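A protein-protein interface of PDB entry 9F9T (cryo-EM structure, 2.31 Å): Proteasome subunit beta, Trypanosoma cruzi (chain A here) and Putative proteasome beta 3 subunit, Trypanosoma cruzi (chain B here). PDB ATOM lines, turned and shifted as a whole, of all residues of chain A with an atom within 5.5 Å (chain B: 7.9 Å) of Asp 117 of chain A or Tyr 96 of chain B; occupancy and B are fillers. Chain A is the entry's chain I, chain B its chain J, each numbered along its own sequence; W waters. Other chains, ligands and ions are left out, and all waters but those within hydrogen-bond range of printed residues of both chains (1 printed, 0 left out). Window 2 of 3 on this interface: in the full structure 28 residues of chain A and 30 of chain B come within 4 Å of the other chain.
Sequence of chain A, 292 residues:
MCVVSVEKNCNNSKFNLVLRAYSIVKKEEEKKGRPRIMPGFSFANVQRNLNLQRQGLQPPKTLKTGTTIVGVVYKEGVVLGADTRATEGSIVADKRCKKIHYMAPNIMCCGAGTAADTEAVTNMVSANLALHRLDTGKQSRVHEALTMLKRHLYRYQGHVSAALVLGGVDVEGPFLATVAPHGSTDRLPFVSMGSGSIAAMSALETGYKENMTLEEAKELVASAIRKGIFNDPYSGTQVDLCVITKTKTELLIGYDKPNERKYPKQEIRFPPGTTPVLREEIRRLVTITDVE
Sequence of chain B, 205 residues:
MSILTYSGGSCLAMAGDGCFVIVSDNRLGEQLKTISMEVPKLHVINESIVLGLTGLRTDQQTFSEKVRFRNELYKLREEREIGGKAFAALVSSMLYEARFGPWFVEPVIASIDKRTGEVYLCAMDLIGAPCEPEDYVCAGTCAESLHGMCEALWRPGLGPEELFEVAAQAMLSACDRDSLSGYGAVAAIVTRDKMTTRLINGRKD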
ATOM      1  N   THR A 114     -12.093  -3.431 -25.272  1.00  0.00           N
ATOM      2  CA  THR A 114     -13.037  -2.428 -25.733  1.00  0.00           C
ATOM      3  C   THR A 114     -12.561  -1.942 -27.082  1.00  0.00           C
ATOM      4  O   THR A 114     -11.442  -1.448 -27.184  1.00  0.00           O
ATOM      5  CB  THR A 114     -13.032  -1.215 -24.780  1.00  0.00           C
ATOM      6  OG1 THR A 114     -12.953  -1.573 -23.400  1.00  0.00           O
ATOM      7  CG2 THR A 114     -14.239  -0.321 -24.940  1.00  0.00           C
ATOM      8  N   ALA A 115     -13.374  -2.063 -28.118  1.00  0.00           N
ATOM      9  CA  ALA A 115     -12.898  -1.736 -29.451  1.00  0.00           C
ATOM     10  C   ALA A 115     -12.408  -0.298 -29.526  1.00  0.00           C
ATOM     11  O   ALA A 115     -11.306  -0.085 -30.019  1.00  0.00           O
ATOM     12  CB  ALA A 115     -13.954  -2.005 -30.462  1.00  0.00           C
ATOM     13  N   ALA A 116     -13.087   0.666 -28.911  1.00  0.00           N
ATOM     14  CA  ALA A 116     -12.653   2.050 -29.110  1.00  0.00           C
ATOM     15  C   ALA A 116     -11.254   2.245 -28.576  1.00  0.00           C
ATOM     16  O   ALA A 116     -10.490   2.903 -29.195  1.00  0.00           O
ATOM     17  CB  ALA A 116     -13.560   3.081 -28.455  1.00  0.00           C
ATOM     18  N   ASP A 117     -11.006   1.733 -27.386  1.00  0.00           N
ATOM     19  CA  ASP A 117      -9.705   1.810 -26.749  1.00  0.00           C
ATOM     20  C   ASP A 117      -8.623   1.067 -27.521  1.00  0.00           C
ATOM     21  O   ASP A 117      -7.541   1.575 -27.711  1.00  0.00           O
ATOM     22  CB  ASP A 117      -9.789   1.264 -25.351  1.00  0.00           C
ATOM     23  CG  ASP A 117     -10.576   2.123 -24.387  1.00  0.00           C
ATOM     24  OD1 ASP A 117     -10.444   3.392 -24.436  1.00  0.00           O
ATOM     25  OD2 ASP A 117     -11.201   1.505 -23.471  1.00  0.00           O
ATOM     26  N   THR A 118      -8.939  -0.098 -28.041  1.00  0.00           N
ATOM     27  CA  THR A 118      -7.960  -0.858 -28.791  1.00  0.00           C
ATOM     28  C   THR A 118      -7.578  -0.103 -30.070  1.00  0.00           C
ATOM     29  O   THR A 118      -6.399   0.010 -30.409  1.00  0.00           O
ATOM     30  CB  THR A 118      -8.502  -2.283 -28.944  1.00  0.00           C
ATOM     31  OG1 THR A 118      -8.603  -2.932 -27.667  1.00  0.00           O
ATOM     32  CG2 THR A 118      -7.621  -3.178 -29.769  1.00  0.00           C
ATOM     33  N   GLU A 119      -8.562   0.445 -30.768  1.00  0.00           N
ATOM     34  CA  GLU A 119      -8.358   1.309 -31.933  1.00  0.00           C
ATOM     35  C   GLU A 119      -7.575   2.570 -31.589  1.00  0.00           C
ATOM     36  O   GLU A 119      -6.579   2.892 -32.209  1.00  0.00           O
ATOM     37  CB  GLU A 119      -9.712   1.824 -32.394  1.00  0.00           C
ATOM     38  CG  GLU A 119     -10.036   1.485 -33.815  1.00  0.00           C
ATOM     39  CD  GLU A 119     -10.621   0.092 -33.986  1.00  0.00           C
ATOM     40  OE1 GLU A 119     -10.071  -0.857 -33.377  1.00  0.00           O
ATOM     41  OE2 GLU A 119     -11.608  -0.044 -34.759  1.00  0.00           O
ATOM     42  N   ALA A 120      -7.942   3.292 -30.544  1.00  0.00           N
ATOM     43  CA  ALA A 120      -7.223   4.518 -30.293  1.00  0.00           C
ATOM     44  C   ALA A 120      -5.736   4.267 -29.992  1.00  0.00           C
ATOM     45  O   ALA A 120      -4.877   4.929 -30.563  1.00  0.00           O
ATOM     46  CB  ALA A 120      -7.915   5.277 -29.186  1.00  0.00           C
ATOM     47  N   VAL A 121      -5.408   3.323 -29.120  1.00  0.00           N
ATOM     48  CA  VAL A 121      -4.035   3.112 -28.765  1.00  0.00           C
ATOM     49  C   VAL A 121      -3.219   2.552 -29.929  1.00  0.00           C
ATOM     50  O   VAL A 121      -2.088   2.935 -30.079  1.00  0.00           O
ATOM     51  CB  VAL A 121      -3.944   2.213 -27.529  1.00  0.00           C
ATOM     52  CG1 VAL A 121      -2.537   1.907 -27.098  1.00  0.00           C
ATOM     53  CG2 VAL A 121      -4.647   2.845 -26.335  1.00  0.00           C
ATOM     54  N   THR A 122      -3.720   1.604 -30.689  1.00  0.00           N
ATOM     55  CA  THR A 122      -2.964   1.136 -31.811  1.00  0.00           C
ATOM     56  C   THR A 122      -2.659   2.243 -32.806  1.00  0.00           C
ATOM     57  O   THR A 122      -1.522   2.343 -33.300  1.00  0.00           O
ATOM     58  CB  THR A 122      -3.727   0.048 -32.588  1.00  0.00           C
ATOM     59  OG1 THR A 122      -5.035   0.532 -32.835  1.00  0.00           O
ATOM     60  CG2 THR A 122      -3.945  -1.195 -31.746  1.00  0.00           C
ATOM     61  N   HIS A 159      -8.015   1.930 -17.334  1.00  0.00           N
ATOM     62  CA  HIS A 159      -9.261   2.573 -17.737  1.00  0.00           C
ATOM     63  C   HIS A 159      -9.361   2.443 -19.250  1.00  0.00           C
ATOM     64  O   HIS A 159     -10.458   2.181 -19.743  1.00  0.00           O
ATOM     65  CB  HIS A 159      -9.430   3.977 -17.136  1.00  0.00           C
ATOM     66  CG  HIS A 159      -9.436   3.911 -15.644  1.00  0.00           C
ATOM     67  ND1 HIS A 159      -9.951   2.792 -15.005  1.00  0.00           N
ATOM     68  CD2 HIS A 159      -8.922   4.696 -14.687  1.00  0.00           C
ATOM     69  CE1 HIS A 159      -9.764   2.911 -13.696  1.00  0.00           C
ATOM     70  NE2 HIS A 159      -9.153   4.067 -13.479  1.00  0.00           N
ATOM     71  N   VAL A 160      -8.213   2.576 -19.937  1.00  0.00           N
ATOM     72  CA  VAL A 160      -8.087   2.329 -21.364  1.00  0.00           C
ATOM     73  C   VAL A 160      -7.928   0.837 -21.507  1.00  0.00           C
ATOM     74  O   VAL A 160      -6.841   0.298 -21.261  1.00  0.00           O
ATOM     75  CB  VAL A 160      -6.873   3.111 -21.948  1.00  0.00           C
ATOM     76  CG1 VAL A 160      -6.545   2.771 -23.409  1.00  0.00           C
ATOM     77  CG2 VAL A 160      -7.045   4.622 -21.756  1.00  0.00           C
ATOM     78  N   SER A 161      -9.014   0.150 -21.848  1.00  0.00           N
ATOM     79  CA  SER A 161      -9.008  -1.287 -21.648  1.00  0.00           C
ATOM     80  C   SER A 161      -8.829  -1.989 -22.984  1.00  0.00           C
ATOM     81  O   SER A 161      -9.668  -2.694 -23.487  1.00  0.00           O
ATOM     82  CB  SER A 161     -10.162  -1.788 -20.742  1.00  0.00           C
ATOM     83  OG  SER A 161     -11.438  -1.602 -21.301  1.00  0.00           O
ATOM     84  N   ALA A 162      -7.611  -1.850 -23.481  1.00  0.00           N
ATOM     85  CA  ALA A 162      -7.091  -2.519 -24.672  1.00  0.00           C
ATOM     86  C   ALA A 162      -6.322  -3.779 -24.285  1.00  0.00           C
ATOM     87  O   ALA A 162      -5.527  -3.802 -23.363  1.00  0.00           O
ATOM     88  CB  ALA A 162      -6.172  -1.540 -25.366  1.00  0.00           C
ATOM     89  N   PHE B  63     -23.926  17.936 -30.162  1.00  0.00           N
ATOM     90  CA  PHE B  63     -22.883  17.297 -30.931  1.00  0.00           C
ATOM     91  C   PHE B  63     -23.062  17.540 -32.408  1.00  0.00           C
ATOM     92  O   PHE B  63     -22.108  17.702 -33.139  1.00  0.00           O
ATOM     93  CB  PHE B  63     -22.926  15.792 -30.701  1.00  0.00           C
ATOM     94  CG  PHE B  63     -21.840  14.988 -31.351  1.00  0.00           C
ATOM     95  CD1 PHE B  63     -20.634  14.830 -30.718  1.00  0.00           C
ATOM     96  CD2 PHE B  63     -22.040  14.408 -32.600  1.00  0.00           C
ATOM     97  CE1 PHE B  63     -19.669  14.052 -31.328  1.00  0.00           C
ATOM     98  CE2 PHE B  63     -20.991  13.794 -33.256  1.00  0.00           C
ATOM     99  CZ  PHE B  63     -19.826  13.582 -32.598  1.00  0.00           C
ATOM    100  N   LEU B  90     -13.523  11.620 -38.378  1.00  0.00           N
ATOM    101  CA  LEU B  90     -13.487  12.845 -37.593  1.00  0.00           C
ATOM    102  C   LEU B  90     -14.442  12.724 -36.418  1.00  0.00           C
ATOM    103  O   LEU B  90     -14.057  13.078 -35.320  1.00  0.00           O
ATOM    104  CB  LEU B  90     -13.886  14.026 -38.474  1.00  0.00           C
ATOM    105  CG  LEU B  90     -14.267  15.297 -37.700  1.00  0.00           C
ATOM    106  CD1 LEU B  90     -13.048  16.030 -37.217  1.00  0.00           C
ATOM    107  CD2 LEU B  90     -15.176  16.222 -38.523  1.00  0.00           C
ATOM    108  N   VAL B  91     -15.689  12.288 -36.713  1.00  0.00           N
ATOM    109  CA  VAL B  91     -16.716  12.035 -35.727  1.00  0.00           C
ATOM    110  C   VAL B  91     -16.227  11.153 -34.601  1.00  0.00           C
ATOM    111  O   VAL B  91     -16.311  11.536 -33.459  1.00  0.00           O
ATOM    112  CB  VAL B  91     -18.001  11.468 -36.321  1.00  0.00           C
ATOM    113  CG1 VAL B  91     -18.857  10.947 -35.202  1.00  0.00           C
ATOM    114  CG2 VAL B  91     -18.865  12.459 -37.036  1.00  0.00           C
ATOM    115  N   SER B  92     -15.582  10.051 -34.953  1.00  0.00           N
ATOM    116  CA  SER B  92     -14.923   9.127 -34.030  1.00  0.00           C
ATOM    117  C   SER B  92     -13.939   9.781 -33.106  1.00  0.00           C
ATOM    118  O   SER B  92     -14.007   9.542 -31.916  1.00  0.00           O
ATOM    119  CB  SER B  92     -14.205   8.112 -34.786  1.00  0.00           C
ATOM    120  OG  SER B  92     -13.759   7.096 -33.929  1.00  0.00           O
ATOM    121  N   SER B  93     -13.060  10.609 -33.665  1.00  0.00           N
ATOM    122  CA  SER B  93     -12.101  11.361 -32.897  1.00  0.00           C
ATOM    123  C   SER B  93     -12.779  12.222 -31.868  1.00  0.00           C
ATOM    124  O   SER B  93     -12.315  12.240 -30.752  1.00  0.00           O
ATOM    125  CB  SER B  93     -11.241  12.235 -33.804  1.00  0.00           C
ATOM    126  OG  SER B  93     -12.018  13.225 -34.475  1.00  0.00           O
ATOM    127  N   MET B  94     -13.819  12.969 -32.238  1.00  0.00           N
ATOM    128  CA  MET B  94     -14.561  13.804 -31.295  1.00  0.00           C
ATOM    129  C   MET B  94     -15.250  12.942 -30.215  1.00  0.00           C
ATOM    130  O   MET B  94     -15.167  13.265 -29.038  1.00  0.00           O
ATOM    131  CB  MET B  94     -15.626  14.667 -31.998  1.00  0.00           C
ATOM    132  CG  MET B  94     -15.098  15.537 -33.081  1.00  0.00           C
ATOM    133  SD  MET B  94     -16.530  16.180 -34.148  1.00  0.00           S
ATOM    134  CE  MET B  94     -17.208  17.476 -33.124  1.00  0.00           C
ATOM    135  N   LEU B  95     -15.924  11.853 -30.561  1.00  0.00           N
ATOM    136  CA  LEU B  95     -16.479  11.058 -29.486  1.00  0.00           C
ATOM    137  C   LEU B  95     -15.386  10.621 -28.522  1.00  0.00           C
ATOM    138  O   LEU B  95     -15.680  10.403 -27.346  1.00  0.00           O
ATOM    139  CB  LEU B  95     -17.229   9.810 -29.979  1.00  0.00           C
ATOM    140  CG  LEU B  95     -18.456  10.167 -30.826  1.00  0.00           C
ATOM    141  CD1 LEU B  95     -19.069   9.003 -31.513  1.00  0.00           C
ATOM    142  CD2 LEU B  95     -19.485  10.883 -30.018  1.00  0.00           C
ATOM    143  N   TYR B  96     -14.207  10.252 -29.011  1.00  0.00           N
ATOM    144  CA  TYR B  96     -13.246   9.632 -28.095  1.00  0.00           C
ATOM    145  C   TYR B  96     -12.522  10.758 -27.347  1.00  0.00           C
ATOM    146  O   TYR B  96     -12.061  10.558 -26.242  1.00  0.00           O
ATOM    147  CB  TYR B  96     -12.312   8.701 -28.874  1.00  0.00           C
ATOM    148  CG  TYR B  96     -11.355   7.864 -28.067  1.00  0.00           C
ATOM    149  CD1 TYR B  96     -11.768   6.642 -27.520  1.00  0.00           C
ATOM    150  CD2 TYR B  96     -10.049   8.284 -27.825  1.00  0.00           C
ATOM    151  CE1 TYR B  96     -10.926   5.868 -26.721  1.00  0.00           C
ATOM    152  CE2 TYR B  96      -9.214   7.530 -26.983  1.00  0.00           C
ATOM    153  CZ  TYR B  96      -9.651   6.326 -26.456  1.00  0.00           C
ATOM    154  OH  TYR B  96      -8.836   5.533 -25.713  1.00  0.00           O
ATOM    155  N   GLU B  97     -12.527  11.990 -27.847  1.00  0.00           N
ATOM    156  CA  GLU B  97     -12.003  13.088 -27.040  1.00  0.00           C
ATOM    157  C   GLU B  97     -12.698  13.082 -25.691  1.00  0.00           C
ATOM    158  O   GLU B  97     -12.143  13.548 -24.712  1.00  0.00           O
ATOM    159  CB  GLU B  97     -12.208  14.504 -27.593  1.00  0.00           C
ATOM    160  CG  GLU B  97     -11.319  14.939 -28.764  1.00  0.00           C
ATOM    161  CD  GLU B  97     -11.757  16.255 -29.439  1.00  0.00           C
ATOM    162  OE1 GLU B  97     -12.035  17.231 -28.684  1.00  0.00           O
ATOM    163  OE2 GLU B  97     -11.824  16.338 -30.724  1.00  0.00           O
ATOM    164  N   ALA B  98     -13.928  12.566 -25.665  1.00  0.00           N
ATOM    165  CA  ALA B  98     -14.766  12.701 -24.494  1.00  0.00           C
ATOM    166  C   ALA B  98     -14.942  11.367 -23.822  1.00  0.00           C
ATOM    167  O   ALA B  98     -15.927  11.178 -23.160  1.00  0.00           O
ATOM    168  CB  ALA B  98     -16.066  13.336 -24.892  1.00  0.00           C
ATOM    169  N   ARG B  99     -13.911  10.539 -23.872  1.00  0.00           N
ATOM    170  CA  ARG B  99     -13.913   9.133 -23.464  1.00  0.00           C
ATOM    171  C   ARG B  99     -14.276   8.873 -21.984  1.00  0.00           C
ATOM    172  O   ARG B  99     -15.012   7.923 -21.651  1.00  0.00           O
ATOM    173  CB  ARG B  99     -12.514   8.615 -23.786  1.00  0.00           C
ATOM    174  CG  ARG B  99     -12.124   7.272 -23.177  1.00  0.00           C
ATOM    175  CD  ARG B  99     -13.024   6.151 -23.664  1.00  0.00           C
ATOM    176  NE  ARG B  99     -12.599   4.846 -23.214  1.00  0.00           N
ATOM    177  CZ  ARG B  99     -13.218   4.179 -22.258  1.00  0.00           C
ATOM    178  NH1 ARG B  99     -12.760   2.987 -21.910  1.00  0.00           N
ATOM    179  NH2 ARG B  99     -14.273   4.713 -21.663  1.00  0.00           N
ATOM    180  N   PHE B 100     -13.846   9.756 -21.088  1.00  0.00           N
ATOM    181  CA  PHE B 100     -14.172   9.561 -19.682  1.00  0.00           C
ATOM    182  C   PHE B 100     -15.381  10.382 -19.237  1.00  0.00           C
ATOM    183  O   PHE B 100     -15.698  10.349 -18.052  1.00  0.00           O
ATOM    184  CB  PHE B 100     -12.907   9.746 -18.842  1.00  0.00           C
ATOM    185  CG  PHE B 100     -11.899   8.671 -19.181  1.00  0.00           C
ATOM    186  CD1 PHE B 100     -12.228   7.327 -19.005  1.00  0.00           C
ATOM    187  CD2 PHE B 100     -10.702   8.985 -19.817  1.00  0.00           C
ATOM    188  CE1 PHE B 100     -11.350   6.326 -19.401  1.00  0.00           C
ATOM    189  CE2 PHE B 100      -9.806   7.988 -20.179  1.00  0.00           C
ATOM    190  CZ  PHE B 100     -10.138   6.663 -19.978  1.00  0.00           C
ATOM    191  N   GLY B 101     -16.105  11.023 -20.176  1.00  0.00           N
ATOM    192  CA  GLY B 101     -17.295  11.828 -19.880  1.00  0.00           C
ATOM    193  C   GLY B 101     -18.057  12.082 -21.171  1.00  0.00           C
ATOM    194  O   GLY B 101     -17.858  13.084 -21.854  1.00  0.00           O
ATOM    195  N   PRO B 102     -18.755  11.042 -21.642  1.00  0.00           N
ATOM    196  CA  PRO B 102     -19.198  10.961 -23.025  1.00  0.00           C
ATOM    197  C   PRO B 102     -20.414  11.775 -23.406  1.00  0.00           C
ATOM    198  O   PRO B 102     -21.229  12.118 -22.565  1.00  0.00           O
ATOM    199  CB  PRO B 102     -19.563   9.488 -23.221  1.00  0.00           C
ATOM    200  CG  PRO B 102     -19.083   8.779 -21.983  1.00  0.00           C
ATOM    201  CD  PRO B 102     -19.045   9.828 -20.899  1.00  0.00           C
ATOM    202  N   TRP B 103     -20.456  12.076 -24.692  1.00  0.00           N
ATOM    203  CA  TRP B 103     -21.650  12.463 -25.370  1.00  0.00           C
ATOM    204  C   TRP B 103     -22.510  11.218 -25.417  1.00  0.00           C
ATOM    205  O   TRP B 103     -22.057  10.163 -25.860  1.00  0.00           O
ATOM    206  CB  TRP B 103     -21.284  12.991 -26.755  1.00  0.00           C
ATOM    207  CG  TRP B 103     -20.339  14.166 -26.755  1.00  0.00           C
ATOM    208  CD1 TRP B 103     -19.025  14.163 -27.154  1.00  0.00           C
ATOM    209  CD2 TRP B 103     -20.598  15.507 -26.320  1.00  0.00           C
ATOM    210  NE1 TRP B 103     -18.458  15.401 -27.010  1.00  0.00           N
ATOM    211  CE2 TRP B 103     -19.400  16.242 -26.495  1.00  0.00           C
ATOM    212  CE3 TRP B 103     -21.723  16.168 -25.827  1.00  0.00           C
ATOM    213  CZ2 TRP B 103     -19.287  17.594 -26.141  1.00  0.00           C
ATOM    214  CZ3 TRP B 103     -21.626  17.505 -25.483  1.00  0.00           C
ATOM    215  CH2 TRP B 103     -20.419  18.207 -25.631  1.00  0.00           C
ATOM    216  N   ASP B 125     -20.562   3.537 -31.407  1.00  0.00           N
ATOM    217  CA  ASP B 125     -20.939   3.562 -30.022  1.00  0.00           C
ATOM    218  C   ASP B 125     -20.664   4.966 -29.519  1.00  0.00           C
ATOM    219  O   ASP B 125     -20.011   5.742 -30.172  1.00  0.00           O
ATOM    220  CB  ASP B 125     -20.195   2.493 -29.205  1.00  0.00           C
ATOM    221  CG  ASP B 125     -18.682   2.706 -29.013  1.00  0.00           C
ATOM    222  OD1 ASP B 125     -18.247   3.857 -28.792  1.00  0.00           O
ATOM    223  OD2 ASP B 125     -17.936   1.703 -28.992  1.00  0.00           O
ATOM    224  N   LEU B 126     -20.929   5.185 -28.264  1.00  0.00           N
ATOM    225  CA  LEU B 126     -20.890   6.508 -27.737  1.00  0.00           C
ATOM    226  C   LEU B 126     -19.466   6.945 -27.420  1.00  0.00           C
ATOM    227  O   LEU B 126     -19.245   8.138 -27.179  1.00  0.00           O
ATOM    228  CB  LEU B 126     -21.857   6.536 -26.543  1.00  0.00           C
ATOM    229  CG  LEU B 126     -21.303   6.113 -25.184  1.00  0.00           C
ATOM    230  CD1 LEU B 126     -22.369   6.230 -24.124  1.00  0.00           C
ATOM    231  CD2 LEU B 126     -20.775   4.701 -25.177  1.00  0.00           C
ATOM    232  N   ILE B 127     -18.466   6.054 -27.512  1.00  0.00           N
ATOM    233  CA  ILE B 127     -17.082   6.528 -27.501  1.00  0.00           C
ATOM    234  C   ILE B 127     -16.379   6.217 -28.801  1.00  0.00           C
ATOM    235  O   ILE B 127     -15.179   6.234 -28.853  1.00  0.00           O
ATOM    236  CB  ILE B 127     -16.300   5.969 -26.312  1.00  0.00           C
ATOM    237  CG1 ILE B 127     -16.074   4.473 -26.441  1.00  0.00           C
ATOM    238  CG2 ILE B 127     -17.025   6.293 -25.010  1.00  0.00           C
ATOM    239  CD1 ILE B 127     -15.184   3.912 -25.340  1.00  0.00           C
ATOM    240  N   GLY B 128     -17.139   6.019 -29.873  1.00  0.00           N
ATOM    241  CA  GLY B 128     -16.614   6.231 -31.208  1.00  0.00           C
ATOM    242  C   GLY B 128     -16.041   4.993 -31.894  1.00  0.00           C
ATOM    243  O   GLY B 128     -15.311   5.137 -32.868  1.00  0.00           O
ATOM    244  N   ALA B 129     -16.362   3.800 -31.399  1.00  0.00           N
ATOM    245  CA  ALA B 129     -15.889   2.575 -32.015  1.00  0.00           C
ATOM    246  C   ALA B 129     -16.703   2.351 -33.245  1.00  0.00           C
ATOM    247  O   ALA B 129     -17.908   2.262 -33.110  1.00  0.00           O
ATOM    248  CB  ALA B 129     -16.019   1.381 -31.084  1.00  0.00           C
HETATM  249  O   HOH W   1     -15.938   0.614 -27.512  1.00  0.00           O
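Water W1 bridges the side-chain carboxylate (OD2) of Asp 125 of chain B and the backbone NH (N) of Ala 116 of chain A.
Asp 117 of chain A touches just these residues of chain B: Tyr 96 and Arg 99.
Of the printed residues of chain A, Tyr 96 of chain B touches Ala 116, Asp 117 and Ala 120.
Ala 116 of chain A touches just these residues of chain B: Tyr 96 (3.9 Å), Ile 127 (3.5 Å) and Ala 129 (3.7 Å).
Printed residues of chain A within 4 Å of Ala 129 of chain B: Ala 116 (3.7 Å).
Of the printed residues of chain A, Phe 100 of chain B touches His 159 (3.8 Å).
Of the printed residues of chain A, Arg 99 of chain B touches Asp 117 (2.7 Å) and His 159 (3.3 Å).
Of the printed residues of chain A, Ile 127 of chain B touches Ala 116.
Of the printed residues of chain B, Ala 120 of chain A touches Tyr 96 (3.4 Å).
The nearest residue of chain A that does not touch Tyr 96 of chain B is Val 160 of chain A (4.3 Å).
The nearest printed residue of chain A that does not touch Ala 129 of chain B is Ala 115 of chain A (4.01 Å).
Tyr 96 of chain B touches Ala 116 of chain A.
Ile 127 of chain B touches Ala 116 of chain A.
N of Ala 116 of chain A touches CB of Ala 129 of chain B (3.7 Å).
Tyr 96 of chain B touches Ala 120 of chain A (CZ to CB, 3.4 Å).
CB of His 159 of chain A touches CE1 of Phe 100 of chain B (3.8 Å).
The backbone NH of Ile 127 of chain B lies within hydrogen-bond range of the side-chain carboxylate of Asp 125 of chain B (2.6 Å).
OD1 of Asp 125 of chain B sits at hydrogen-bond distance from N of Ala 129 of chain B (3.2 Å).
OD2 of Asp 117 of chain A sits at hydrogen-bond distance from N of Ser 161 of chain A (3.0 Å).
OH of Tyr 96 of chain B sits at hydrogen-bond distance from OD1 of Asp 117 of chain A (3.0 Å).
The guanidinium group (NH1) of Arg 99 of chain B is in salt-bridge range of the side-chain carboxylate (OD2) of Asp 117 of chain A, at 2.7 Å.
The backbone carbonyl oxygen (O) of His 159 of chain A sits at hydrogen-bond distance from the guanidinium group (NH1) of Arg 99 of chain B, at 3.3 Å.
Of the 13 printed residues of chain A, 4 touch a printed residue of chain B.
Printed residues of chain B that touch a printed residue of chain A: Tyr 96, Arg 99, Phe 100, Ile 127 and Ala 129.
Hydrophobic or aromatic side chains of chain B that line the printed part of chain A: Tyr 96, Phe 100, Ile 127 and Ala 129.
Among the printed residues, 8 pairs touch across the chains.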
